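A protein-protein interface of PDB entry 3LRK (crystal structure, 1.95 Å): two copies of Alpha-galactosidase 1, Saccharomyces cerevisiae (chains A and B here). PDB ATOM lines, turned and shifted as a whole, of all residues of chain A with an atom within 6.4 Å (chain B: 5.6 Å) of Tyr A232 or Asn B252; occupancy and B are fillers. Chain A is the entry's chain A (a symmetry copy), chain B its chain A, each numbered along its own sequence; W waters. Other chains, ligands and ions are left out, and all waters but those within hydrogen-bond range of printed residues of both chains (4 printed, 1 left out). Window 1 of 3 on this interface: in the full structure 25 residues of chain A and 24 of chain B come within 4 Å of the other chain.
The side-chain hydroxyl (OH) of Tyr B228 is in hydrogen-bond range of the side-chain sulfur (SG) of Cys A223 (3.5 Å).
The backbone carbonyl oxygen (O) of Pro B248 sits at hydrogen-bond distance from the side-chain hydroxyl (OH) of Tyr A232, at 3.1 Å.
The side-chain amide oxygen (OE1) of Gln B251 lies close to the backbone carbonyl oxygen (O) of Arg A220, 2.9 Å away.
The side-chain amide oxygen of Asn B252 is in hydrogen-bond range of the side-chain hydroxyl of Tyr A232.
The backbone carbonyl oxygen (O) of Arg A220 sits at hydrogen-bond distance from the backbone NH (N) of Phe A235, 3.0 Å away.
The backbone carbonyl oxygen (O) of Phe A235 sits close to the backbone NH (N) of Cys A221 (3.4 Å).
The side-chain sulfur (SG) of Cys A223 is disulfide-bonded to the side-chain sulfur (SG) of Cys A230.
O of Cys A223 is in hydrogen-bond range of NZ of Lys A245 (3.0 Å).
N of Tyr A232 sits close to SG of Cys A230 (3.4 Å).
The side-chain sulfur (SG) of Cys A230 is in hydrogen-bond range of the backbone NH (N) of Ala A233, 3.6 Å away.
CE2 of Tyr A152 touches OG of Ser B198 (3.6 Å).
Pro A222 touches Pro B248 (CG to CB, 3.9 Å).
O of Lys A231 touches CE1 of Tyr B195, 3.6 Å away.
Tyr A232 touches Phe B194 (CZ to CE1, 3.3 Å).
Tyr B195 touches Tyr A232.
CB of Tyr A232 touches CE1 of Tyr B228, 3.5 Å away.
Met B249 touches Tyr A232 (CA to OH, 3.3 Å).
Tyr A232 touches Gln B251.
N of Ala A233 touches OH of Tyr B195 (3.5 Å).
Gln B251 touches Phe A235 (NE2 to CD2, 3.1 Å).
Of chain B, only Phe B194, Tyr B195, Tyr B228, Pro B248, Met B249, Gln B251 and Asn B252 come within 4 Å of Tyr A232.
Asn B252 touches just one residue of chain A: Tyr A232.
Of the printed residues of chain B, Lys A231 touches Tyr B195 (3.6 Å).
Printed residues of chain A within 4 Å of Tyr B195: Lys A231 (3.6 Å), Tyr A232 (3.6 Å) and Ala A233 (3.5 Å).
Of the printed residues of chain A, Pro B248 touches Pro A222 (3.9 Å) and Tyr A232 (3.1 Å).
The nearest residue of chain A that does not touch Asn B252 is Tyr A152 (6.1 Å).
The nearest printed residue of chain A that does not touch Gln B251 is Cys A221 (4.9 Å).
Of the 13 printed residues of chain A, 9 touch a printed residue of chain B.
Printed residues of chain A that touch a printed residue of chain B: Tyr A152, Arg A220, Pro A222, Cys A223, Lys A231, Tyr A232, Ala A233, Gly A234 and Phe A235.
Among the printed residues, 16 pairs touch across the chains.
Among the printed residues, no Asp or Glu carboxylate lies within 4 Å of a Lys or Arg side-chain nitrogen of the other chain.
No position is printed for both chains.
Water W4 lies within hydrogen-bond range of the side-chain carboxylate of Glu A227, the backbone NH of Lys A231, the side-chain hydroxyl of Tyr B228 and the side-chain sulfur of Cys A223.
Water W1 lies within hydrogen-bond range of the backbone carbonyl oxygen of Tyr B195 (2.7 Å) and the backbone NH of Tyr A152 (3.3 Å).
Water W2 bridges OH of Tyr B195 and N of Gly A234.
Water W3 bridges OH of Tyr B195 (3.0 Å) and N of Ala A233 (3.0 Å).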
ATOM      1  N   TYR A 152      11.239 -17.856 -27.348  1.00  0.00           N
ATOM      2  CA  TYR A 152      10.305 -17.023 -28.130  1.00  0.00           C
ATOM      3  C   TYR A 152      10.270 -17.331 -29.626  1.00  0.00           C
ATOM      4  O   TYR A 152      10.325 -16.429 -30.475  1.00  0.00           O
ATOM      5  CB  TYR A 152      10.554 -15.528 -27.830  1.00  0.00           C
ATOM      6  CG  TYR A 152      10.460 -15.295 -26.343  1.00  0.00           C
ATOM      7  CD1 TYR A 152      11.604 -15.039 -25.584  1.00  0.00           C
ATOM      8  CD2 TYR A 152       9.229 -15.391 -25.685  1.00  0.00           C
ATOM      9  CE1 TYR A 152      11.528 -14.868 -24.202  1.00  0.00           C
ATOM     10  CE2 TYR A 152       9.138 -15.220 -24.296  1.00  0.00           C
ATOM     11  CZ  TYR A 152      10.291 -14.942 -23.571  1.00  0.00           C
ATOM     12  OH  TYR A 152      10.222 -14.787 -22.207  1.00  0.00           O
ATOM     13  N   ARG A 220      11.023 -28.047 -12.588  1.00  0.00           N
ATOM     14  CA  ARG A 220      11.308 -27.234 -13.780  1.00  0.00           C
ATOM     15  C   ARG A 220      11.957 -28.047 -14.911  1.00  0.00           C
ATOM     16  O   ARG A 220      12.121 -27.540 -16.022  1.00  0.00           O
ATOM     17  CB  ARG A 220      12.188 -26.026 -13.417  1.00  0.00           C
ATOM     18  CG  ARG A 220      11.506 -25.021 -12.481  1.00  0.00           C
ATOM     19  CD  ARG A 220      12.525 -24.093 -11.824  1.00  0.00           C
ATOM     20  NE  ARG A 220      13.404 -24.803 -10.889  1.00  0.00           N
ATOM     21  CZ  ARG A 220      14.323 -24.212 -10.131  1.00  0.00           C
ATOM     22  NH1 ARG A 220      14.493 -22.898 -10.198  1.00  0.00           N
ATOM     23  NH2 ARG A 220      15.080 -24.931  -9.304  1.00  0.00           N
ATOM     24  N   CYS A 221      12.316 -29.296 -14.610  1.00  0.00           N
ATOM     25  CA  CYS A 221      12.877 -30.240 -15.585  1.00  0.00           C
ATOM     26  C   CYS A 221      12.047 -31.533 -15.566  1.00  0.00           C
ATOM     27  O   CYS A 221      12.504 -32.566 -15.060  1.00  0.00           O
ATOM     28  CB  CYS A 221      14.354 -30.505 -15.278  1.00  0.00           C
ATOM     29  SG  CYS A 221      15.242 -31.609 -16.420  1.00  0.00           S
ATOM     30  N   PRO A 222      10.804 -31.476 -16.104  1.00  0.00           N
ATOM     31  CA  PRO A 222       9.843 -32.572 -15.909  1.00  0.00           C
ATOM     32  C   PRO A 222      10.182 -33.904 -16.602  1.00  0.00           C
ATOM     33  O   PRO A 222       9.641 -34.942 -16.206  1.00  0.00           O
ATOM     34  CB  PRO A 222       8.527 -31.984 -16.442  1.00  0.00           C
ATOM     35  CG  PRO A 222       8.951 -31.011 -17.476  1.00  0.00           C
ATOM     36  CD  PRO A 222      10.229 -30.394 -16.929  1.00  0.00           C
ATOM     37  N   CYS A 223      11.061 -33.885 -17.601  1.00  0.00           N
ATOM     38  CA  CYS A 223      11.450 -35.118 -18.295  1.00  0.00           C
ATOM     39  C   CYS A 223      12.576 -35.807 -17.548  1.00  0.00           C
ATOM     40  O   CYS A 223      13.626 -35.204 -17.317  1.00  0.00           O
ATOM     41  CB  CYS A 223      11.875 -34.822 -19.732  1.00  0.00           C
ATOM     42  SG  CYS A 223      10.575 -34.136 -20.744  1.00  0.00           S
ATOM     43  N   GLU A 227      13.687 -40.002 -20.664  1.00  0.00           N
ATOM     44  CA  GLU A 227      12.877 -39.269 -21.642  1.00  0.00           C
ATOM     45  C   GLU A 227      13.739 -38.379 -22.545  1.00  0.00           C
ATOM     46  O   GLU A 227      13.709 -37.145 -22.439  1.00  0.00           O
ATOM     47  CB  GLU A 227      11.731 -38.495 -20.956  1.00  0.00           C
ATOM     48  CG  GLU A 227      10.567 -38.155 -21.912  1.00  0.00           C
ATOM     49  CD  GLU A 227       9.383 -37.480 -21.228  1.00  0.00           C
ATOM     50  OE1 GLU A 227       9.373 -37.351 -19.985  1.00  0.00           O
ATOM     51  OE2 GLU A 227       8.447 -37.090 -21.951  1.00  0.00           O
ATOM     52  N   CYS A 230      11.838 -35.366 -25.297  1.00  0.00           N
ATOM     53  CA  CYS A 230      11.136 -34.628 -24.260  1.00  0.00           C
ATOM     54  C   CYS A 230      10.367 -33.468 -24.884  1.00  0.00           C
ATOM     55  O   CYS A 230      10.897 -32.775 -25.749  1.00  0.00           O
ATOM     56  CB  CYS A 230      12.178 -34.099 -23.265  1.00  0.00           C
ATOM     57  SG  CYS A 230      11.558 -32.951 -22.047  1.00  0.00           S
ATOM     58  N   LYS A 231       9.129 -33.239 -24.437  1.00  0.00           N
ATOM     59  CA  LYS A 231       8.302 -32.172 -25.006  1.00  0.00           C
ATOM     60  C   LYS A 231       8.337 -30.864 -24.204  1.00  0.00           C
ATOM     61  O   LYS A 231       7.761 -29.848 -24.615  1.00  0.00           O
ATOM     62  CB  LYS A 231       6.856 -32.653 -25.210  1.00  0.00           C
ATOM     63  CG  LYS A 231       6.714 -33.899 -26.133  1.00  0.00           C
ATOM     64  CD  LYS A 231       7.099 -33.601 -27.585  1.00  0.00           C
ATOM     65  CE  LYS A 231       6.668 -34.751 -28.501  1.00  0.00           C
ATOM     66  NZ  LYS A 231       7.063 -34.532 -29.929  1.00  0.00           N
ATOM     67  N   TYR A 232       9.014 -30.894 -23.065  1.00  0.00           N
ATOM     68  CA  TYR A 232       9.209 -29.701 -22.247  1.00  0.00           C
ATOM     69  C   TYR A 232      10.591 -29.791 -21.625  1.00  0.00           C
ATOM     70  O   TYR A 232      10.728 -30.259 -20.497  1.00  0.00           O
ATOM     71  CB  TYR A 232       8.149 -29.616 -21.139  1.00  0.00           C
ATOM     72  CG  TYR A 232       7.934 -28.232 -20.555  1.00  0.00           C
ATOM     73  CD1 TYR A 232       6.814 -27.962 -19.755  1.00  0.00           C
ATOM     74  CD2 TYR A 232       8.826 -27.185 -20.812  1.00  0.00           C
ATOM     75  CE1 TYR A 232       6.595 -26.680 -19.229  1.00  0.00           C
ATOM     76  CE2 TYR A 232       8.624 -25.914 -20.290  1.00  0.00           C
ATOM     77  CZ  TYR A 232       7.501 -25.664 -19.502  1.00  0.00           C
ATOM     78  OH  TYR A 232       7.294 -24.395 -19.001  1.00  0.00           O
ATOM     79  N   ALA A 233      11.613 -29.372 -22.373  1.00  0.00           N
ATOM     80  CA  ALA A 233      13.010 -29.520 -21.943  1.00  0.00           C
ATOM     81  C   ALA A 233      13.285 -28.890 -20.573  1.00  0.00           C
ATOM     82  O   ALA A 233      13.979 -29.481 -19.727  1.00  0.00           O
ATOM     83  CB  ALA A 233      13.956 -28.951 -22.990  1.00  0.00           C
ATOM     84  N   GLY A 234      12.725 -27.703 -20.372  1.00  0.00           N
ATOM     85  CA  GLY A 234      12.814 -26.989 -19.101  1.00  0.00           C
ATOM     86  C   GLY A 234      14.245 -26.627 -18.758  1.00  0.00           C
ATOM     87  O   GLY A 234      15.069 -26.413 -19.653  1.00  0.00           O
ATOM     88  N   PHE A 235      14.538 -26.573 -17.458  1.00  0.00           N
ATOM     89  CA  PHE A 235      15.886 -26.279 -16.957  1.00  0.00           C
ATOM     90  C   PHE A 235      16.038 -26.711 -15.497  1.00  0.00           C
ATOM     91  O   PHE A 235      15.130 -27.339 -14.945  1.00  0.00           O
ATOM     92  CB  PHE A 235      16.329 -24.816 -17.222  1.00  0.00           C
ATOM     93  CG  PHE A 235      15.596 -23.749 -16.419  1.00  0.00           C
ATOM     94  CD1 PHE A 235      16.269 -22.580 -16.055  1.00  0.00           C
ATOM     95  CD2 PHE A 235      14.263 -23.885 -16.047  1.00  0.00           C
ATOM     96  CE1 PHE A 235      15.621 -21.566 -15.323  1.00  0.00           C
ATOM     97  CE2 PHE A 235      13.603 -22.875 -15.329  1.00  0.00           C
ATOM     98  CZ  PHE A 235      14.288 -21.717 -14.960  1.00  0.00           C
ATOM     99  N   LYS A 245      19.811 -38.742 -20.463  1.00  0.00           N
ATOM    100  CA  LYS A 245      19.231 -38.289 -21.732  1.00  0.00           C
ATOM    101  C   LYS A 245      20.200 -38.438 -22.920  1.00  0.00           C
ATOM    102  O   LYS A 245      19.788 -38.829 -24.022  1.00  0.00           O
ATOM    103  CB  LYS A 245      18.733 -36.849 -21.599  1.00  0.00           C
ATOM    104  CG  LYS A 245      17.422 -36.753 -20.841  1.00  0.00           C
ATOM    105  CD  LYS A 245      17.101 -35.325 -20.470  1.00  0.00           C
ATOM    106  CE  LYS A 245      15.723 -35.234 -19.844  1.00  0.00           C
ATOM    107  NZ  LYS A 245      15.585 -33.908 -19.172  1.00  0.00           N
ATOM    108  N   PHE B 194       1.963 -22.933 -23.606  1.00  0.00           N
ATOM    109  CA  PHE B 194       2.897 -22.155 -22.761  1.00  0.00           C
ATOM    110  C   PHE B 194       4.149 -21.691 -23.531  1.00  0.00           C
ATOM    111  O   PHE B 194       4.793 -20.690 -23.165  1.00  0.00           O
ATOM    112  CB  PHE B 194       3.298 -22.965 -21.507  1.00  0.00           C
ATOM    113  CG  PHE B 194       4.054 -24.233 -21.826  1.00  0.00           C
ATOM    114  CD1 PHE B 194       5.420 -24.190 -22.126  1.00  0.00           C
ATOM    115  CD2 PHE B 194       3.396 -25.461 -21.845  1.00  0.00           C
ATOM    116  CE1 PHE B 194       6.108 -25.341 -22.453  1.00  0.00           C
ATOM    117  CE2 PHE B 194       4.085 -26.624 -22.167  1.00  0.00           C
ATOM    118  CZ  PHE B 194       5.449 -26.556 -22.470  1.00  0.00           C
ATOM    119  N   TYR B 195       4.496 -22.422 -24.596  1.00  0.00           N
ATOM    120  CA  TYR B 195       5.667 -22.074 -25.405  1.00  0.00           C
ATOM    121  C   TYR B 195       5.400 -20.906 -26.373  1.00  0.00           C
ATOM    122  O   TYR B 195       6.295 -20.090 -26.623  1.00  0.00           O
ATOM    123  CB  TYR B 195       6.133 -23.288 -26.216  1.00  0.00           C
ATOM    124  CG  TYR B 195       7.224 -24.143 -25.609  1.00  0.00           C
ATOM    125  CD1 TYR B 195       7.162 -25.534 -25.716  1.00  0.00           C
ATOM    126  CD2 TYR B 195       8.332 -23.579 -24.960  1.00  0.00           C
ATOM    127  CE1 TYR B 195       8.147 -26.344 -25.207  1.00  0.00           C
ATOM    128  CE2 TYR B 195       9.349 -24.402 -24.440  1.00  0.00           C
ATOM    129  CZ  TYR B 195       9.240 -25.782 -24.568  1.00  0.00           C
ATOM    130  OH  TYR B 195      10.213 -26.632 -24.069  1.00  0.00           O
ATOM    131  N   SER B 198       2.821 -16.278 -25.466  1.00  0.00           N
ATOM    132  CA  SER B 198       3.243 -14.933 -25.015  1.00  0.00           C
ATOM    133  C   SER B 198       3.315 -13.863 -26.107  1.00  0.00           C
ATOM    134  O   SER B 198       2.975 -12.692 -25.866  1.00  0.00           O
ATOM    135  CB  SER B 198       4.559 -14.996 -24.228  1.00  0.00           C
ATOM    136  OG  SER B 198       5.655 -15.281 -25.078  1.00  0.00           O
ATOM    137  N   TRP B 204      -3.284 -17.796 -21.222  1.00  0.00           N
ATOM    138  CA  TRP B 204      -3.708 -19.030 -21.902  1.00  0.00           C
ATOM    139  C   TRP B 204      -4.122 -20.079 -20.889  1.00  0.00           C
ATOM    140  O   TRP B 204      -3.374 -20.400 -19.960  1.00  0.00           O
ATOM    141  CB  TRP B 204      -2.595 -19.587 -22.815  1.00  0.00           C
ATOM    142  CG  TRP B 204      -1.255 -19.564 -22.185  1.00  0.00           C
ATOM    143  CD1 TRP B 204      -0.690 -20.545 -21.432  1.00  0.00           C
ATOM    144  CD2 TRP B 204      -0.304 -18.480 -22.217  1.00  0.00           C
ATOM    145  NE1 TRP B 204       0.561 -20.154 -21.001  1.00  0.00           N
ATOM    146  CE2 TRP B 204       0.818 -18.890 -21.463  1.00  0.00           C
ATOM    147  CE3 TRP B 204      -0.293 -17.213 -22.813  1.00  0.00           C
ATOM    148  CZ2 TRP B 204       1.951 -18.074 -21.283  1.00  0.00           C
ATOM    149  CZ3 TRP B 204       0.842 -16.387 -22.621  1.00  0.00           C
ATOM    150  CH2 TRP B 204       1.942 -16.837 -21.871  1.00  0.00           C
ATOM    151  N   TYR B 228       1.278 -32.978 -18.448  1.00  0.00           N
ATOM    152  CA  TYR B 228       1.184 -31.569 -18.853  1.00  0.00           C
ATOM    153  C   TYR B 228       1.003 -31.413 -20.361  1.00  0.00           C
ATOM    154  O   TYR B 228       0.416 -30.442 -20.819  1.00  0.00           O
ATOM    155  CB  TYR B 228       2.428 -30.781 -18.393  1.00  0.00           C
ATOM    156  CG  TYR B 228       3.721 -31.408 -18.867  1.00  0.00           C
ATOM    157  CD1 TYR B 228       4.264 -31.080 -20.108  1.00  0.00           C
ATOM    158  CD2 TYR B 228       4.384 -32.351 -18.085  1.00  0.00           C
ATOM    159  CE1 TYR B 228       5.446 -31.681 -20.562  1.00  0.00           C
ATOM    160  CE2 TYR B 228       5.562 -32.953 -18.525  1.00  0.00           C
ATOM    161  CZ  TYR B 228       6.085 -32.609 -19.762  1.00  0.00           C
ATOM    162  OH  TYR B 228       7.238 -33.208 -20.199  1.00  0.00           O
ATOM    163  N   PRO B 248       5.279 -27.474 -13.946  1.00  0.00           N
ATOM    164  CA  PRO B 248       6.463 -27.196 -14.769  1.00  0.00           C
ATOM    165  C   PRO B 248       6.338 -25.927 -15.627  1.00  0.00           C
ATOM    166  O   PRO B 248       7.347 -25.422 -16.096  1.00  0.00           O
ATOM    167  CB  PRO B 248       6.562 -28.440 -15.670  1.00  0.00           C
ATOM    168  CG  PRO B 248       5.168 -28.919 -15.793  1.00  0.00           C
ATOM    169  CD  PRO B 248       4.543 -28.663 -14.435  1.00  0.00           C
ATOM    170  N   MET B 249       5.117 -25.408 -15.788  1.00  0.00           N
ATOM    171  CA  MET B 249       4.837 -24.308 -16.733  1.00  0.00           C
ATOM    172  C   MET B 249       5.160 -22.898 -16.252  1.00  0.00           C
ATOM    173  O   MET B 249       5.169 -21.966 -17.056  1.00  0.00           O
ATOM    174  CB  MET B 249       3.383 -24.345 -17.188  1.00  0.00           C
ATOM    175  CG  MET B 249       2.977 -25.658 -17.870  1.00  0.00           C
ATOM    176  SD  MET B 249       1.274 -25.449 -18.373  1.00  0.00           S
ATOM    177  CE  MET B 249       0.858 -27.095 -18.975  1.00  0.00           C
ATOM    178  N   GLY B 250       5.421 -22.739 -14.958  1.00  0.00           N
ATOM    179  CA  GLY B 250       5.724 -21.415 -14.389  1.00  0.00           C
ATOM    180  C   GLY B 250       6.858 -20.689 -15.091  1.00  0.00           C
ATOM    181  O   GLY B 250       6.827 -19.469 -15.256  1.00  0.00           O
ATOM    182  N   GLN B 251       7.863 -21.453 -15.508  1.00  0.00           N
ATOM    183  CA  GLN B 251       9.038 -20.913 -16.183  1.00  0.00           C
ATOM    184  C   GLN B 251       8.733 -20.251 -17.527  1.00  0.00           C
ATOM    185  O   GLN B 251       9.548 -19.486 -18.032  1.00  0.00           O
ATOM    186  CB  GLN B 251      10.097 -22.013 -16.373  1.00  0.00           C
ATOM    187  CG  GLN B 251       9.653 -23.134 -17.308  1.00  0.00           C
ATOM    188  CD  GLN B 251      10.580 -24.332 -17.264  1.00  0.00           C
ATOM    189  OE1 GLN B 251      10.247 -25.370 -16.692  1.00  0.00           O
ATOM    190  NE2 GLN B 251      11.747 -24.190 -17.854  1.00  0.00           N
ATOM    191  N   ASN B 252       7.569 -20.563 -18.103  1.00  0.00           N
ATOM    192  CA  ASN B 252       7.130 -19.959 -19.355  1.00  0.00           C
ATOM    193  C   ASN B 252       6.039 -18.903 -19.193  1.00  0.00           C
ATOM    194  O   ASN B 252       5.448 -18.462 -20.174  1.00  0.00           O
ATOM    195  CB  ASN B 252       6.724 -21.038 -20.373  1.00  0.00           C
ATOM    196  CG  ASN B 252       7.919 -21.594 -21.124  1.00  0.00           C
ATOM    197  OD1 ASN B 252       8.515 -22.573 -20.701  1.00  0.00           O
ATOM    198  ND2 ASN B 252       8.301 -20.936 -22.221  1.00  0.00           N
ATOM    199  N   ALA B 253       5.808 -18.470 -17.955  1.00  0.00           N
ATOM    200  CA  ALA B 253       4.926 -17.336 -17.689  1.00  0.00           C
ATOM    201  C   ALA B 253       5.674 -16.138 -17.084  1.00  0.00           C
ATOM    202  O   ALA B 253       6.794 -16.271 -16.594  1.00  0.00           O
ATOM    203  CB  ALA B 253       3.775 -17.759 -16.799  1.00  0.00           C
ATOM    204  N   GLY B 254       5.036 -14.973 -17.126  1.00  0.00           N
ATOM    205  CA  GLY B 254       5.611 -13.748 -16.578  1.00  0.00           C
ATOM    206  C   GLY B 254       4.906 -12.522 -17.124  1.00  0.00           C
ATOM    207  O   GLY B 254       3.913 -12.642 -17.841  1.00  0.00           O
ATOM    208  N   GLY B 257       2.071 -12.242 -20.060  1.00  0.00           N
ATOM    209  CA  GLY B 257       1.587 -13.535 -20.572  1.00  0.00           C
ATOM    210  C   GLY B 257       1.596 -14.594 -19.482  1.00  0.00           C
ATOM    211  O   GLY B 257       2.656 -15.022 -19.045  1.00  0.00           O
ATOM    212  N   ASN B 259       0.043 -18.252 -17.444  1.00  0.00           N
ATOM    213  CA  ASN B 259      -0.680 -19.516 -17.397  1.00  0.00           C
ATOM    214  C   ASN B 259      -2.017 -19.271 -16.691  1.00  0.00           C
ATOM    215  O   ASN B 259      -2.081 -18.527 -15.708  1.00  0.00           O
ATOM    216  CB  ASN B 259       0.121 -20.570 -16.635  1.00  0.00           C
ATOM    217  CG  ASN B 259       1.423 -20.949 -17.341  1.00  0.00           C
ATOM    218  OD1 ASN B 259       1.441 -21.204 -18.542  1.00  0.00           O
ATOM    219  ND2 ASN B 259       2.511 -21.006 -16.584  1.00  0.00           N
HETATM  220  O   HOH W   1       8.811 -20.098 -27.553  1.00  0.00           O
HETATM  221  O   HOH W   2      11.847 -25.572 -22.154  1.00  0.00           O
HETATM  222  O   HOH W   3      11.314 -29.112 -25.380  1.00  0.00           O
HETATM  223  O   HOH W   4       7.535 -34.717 -22.624  1.00  0.00           O
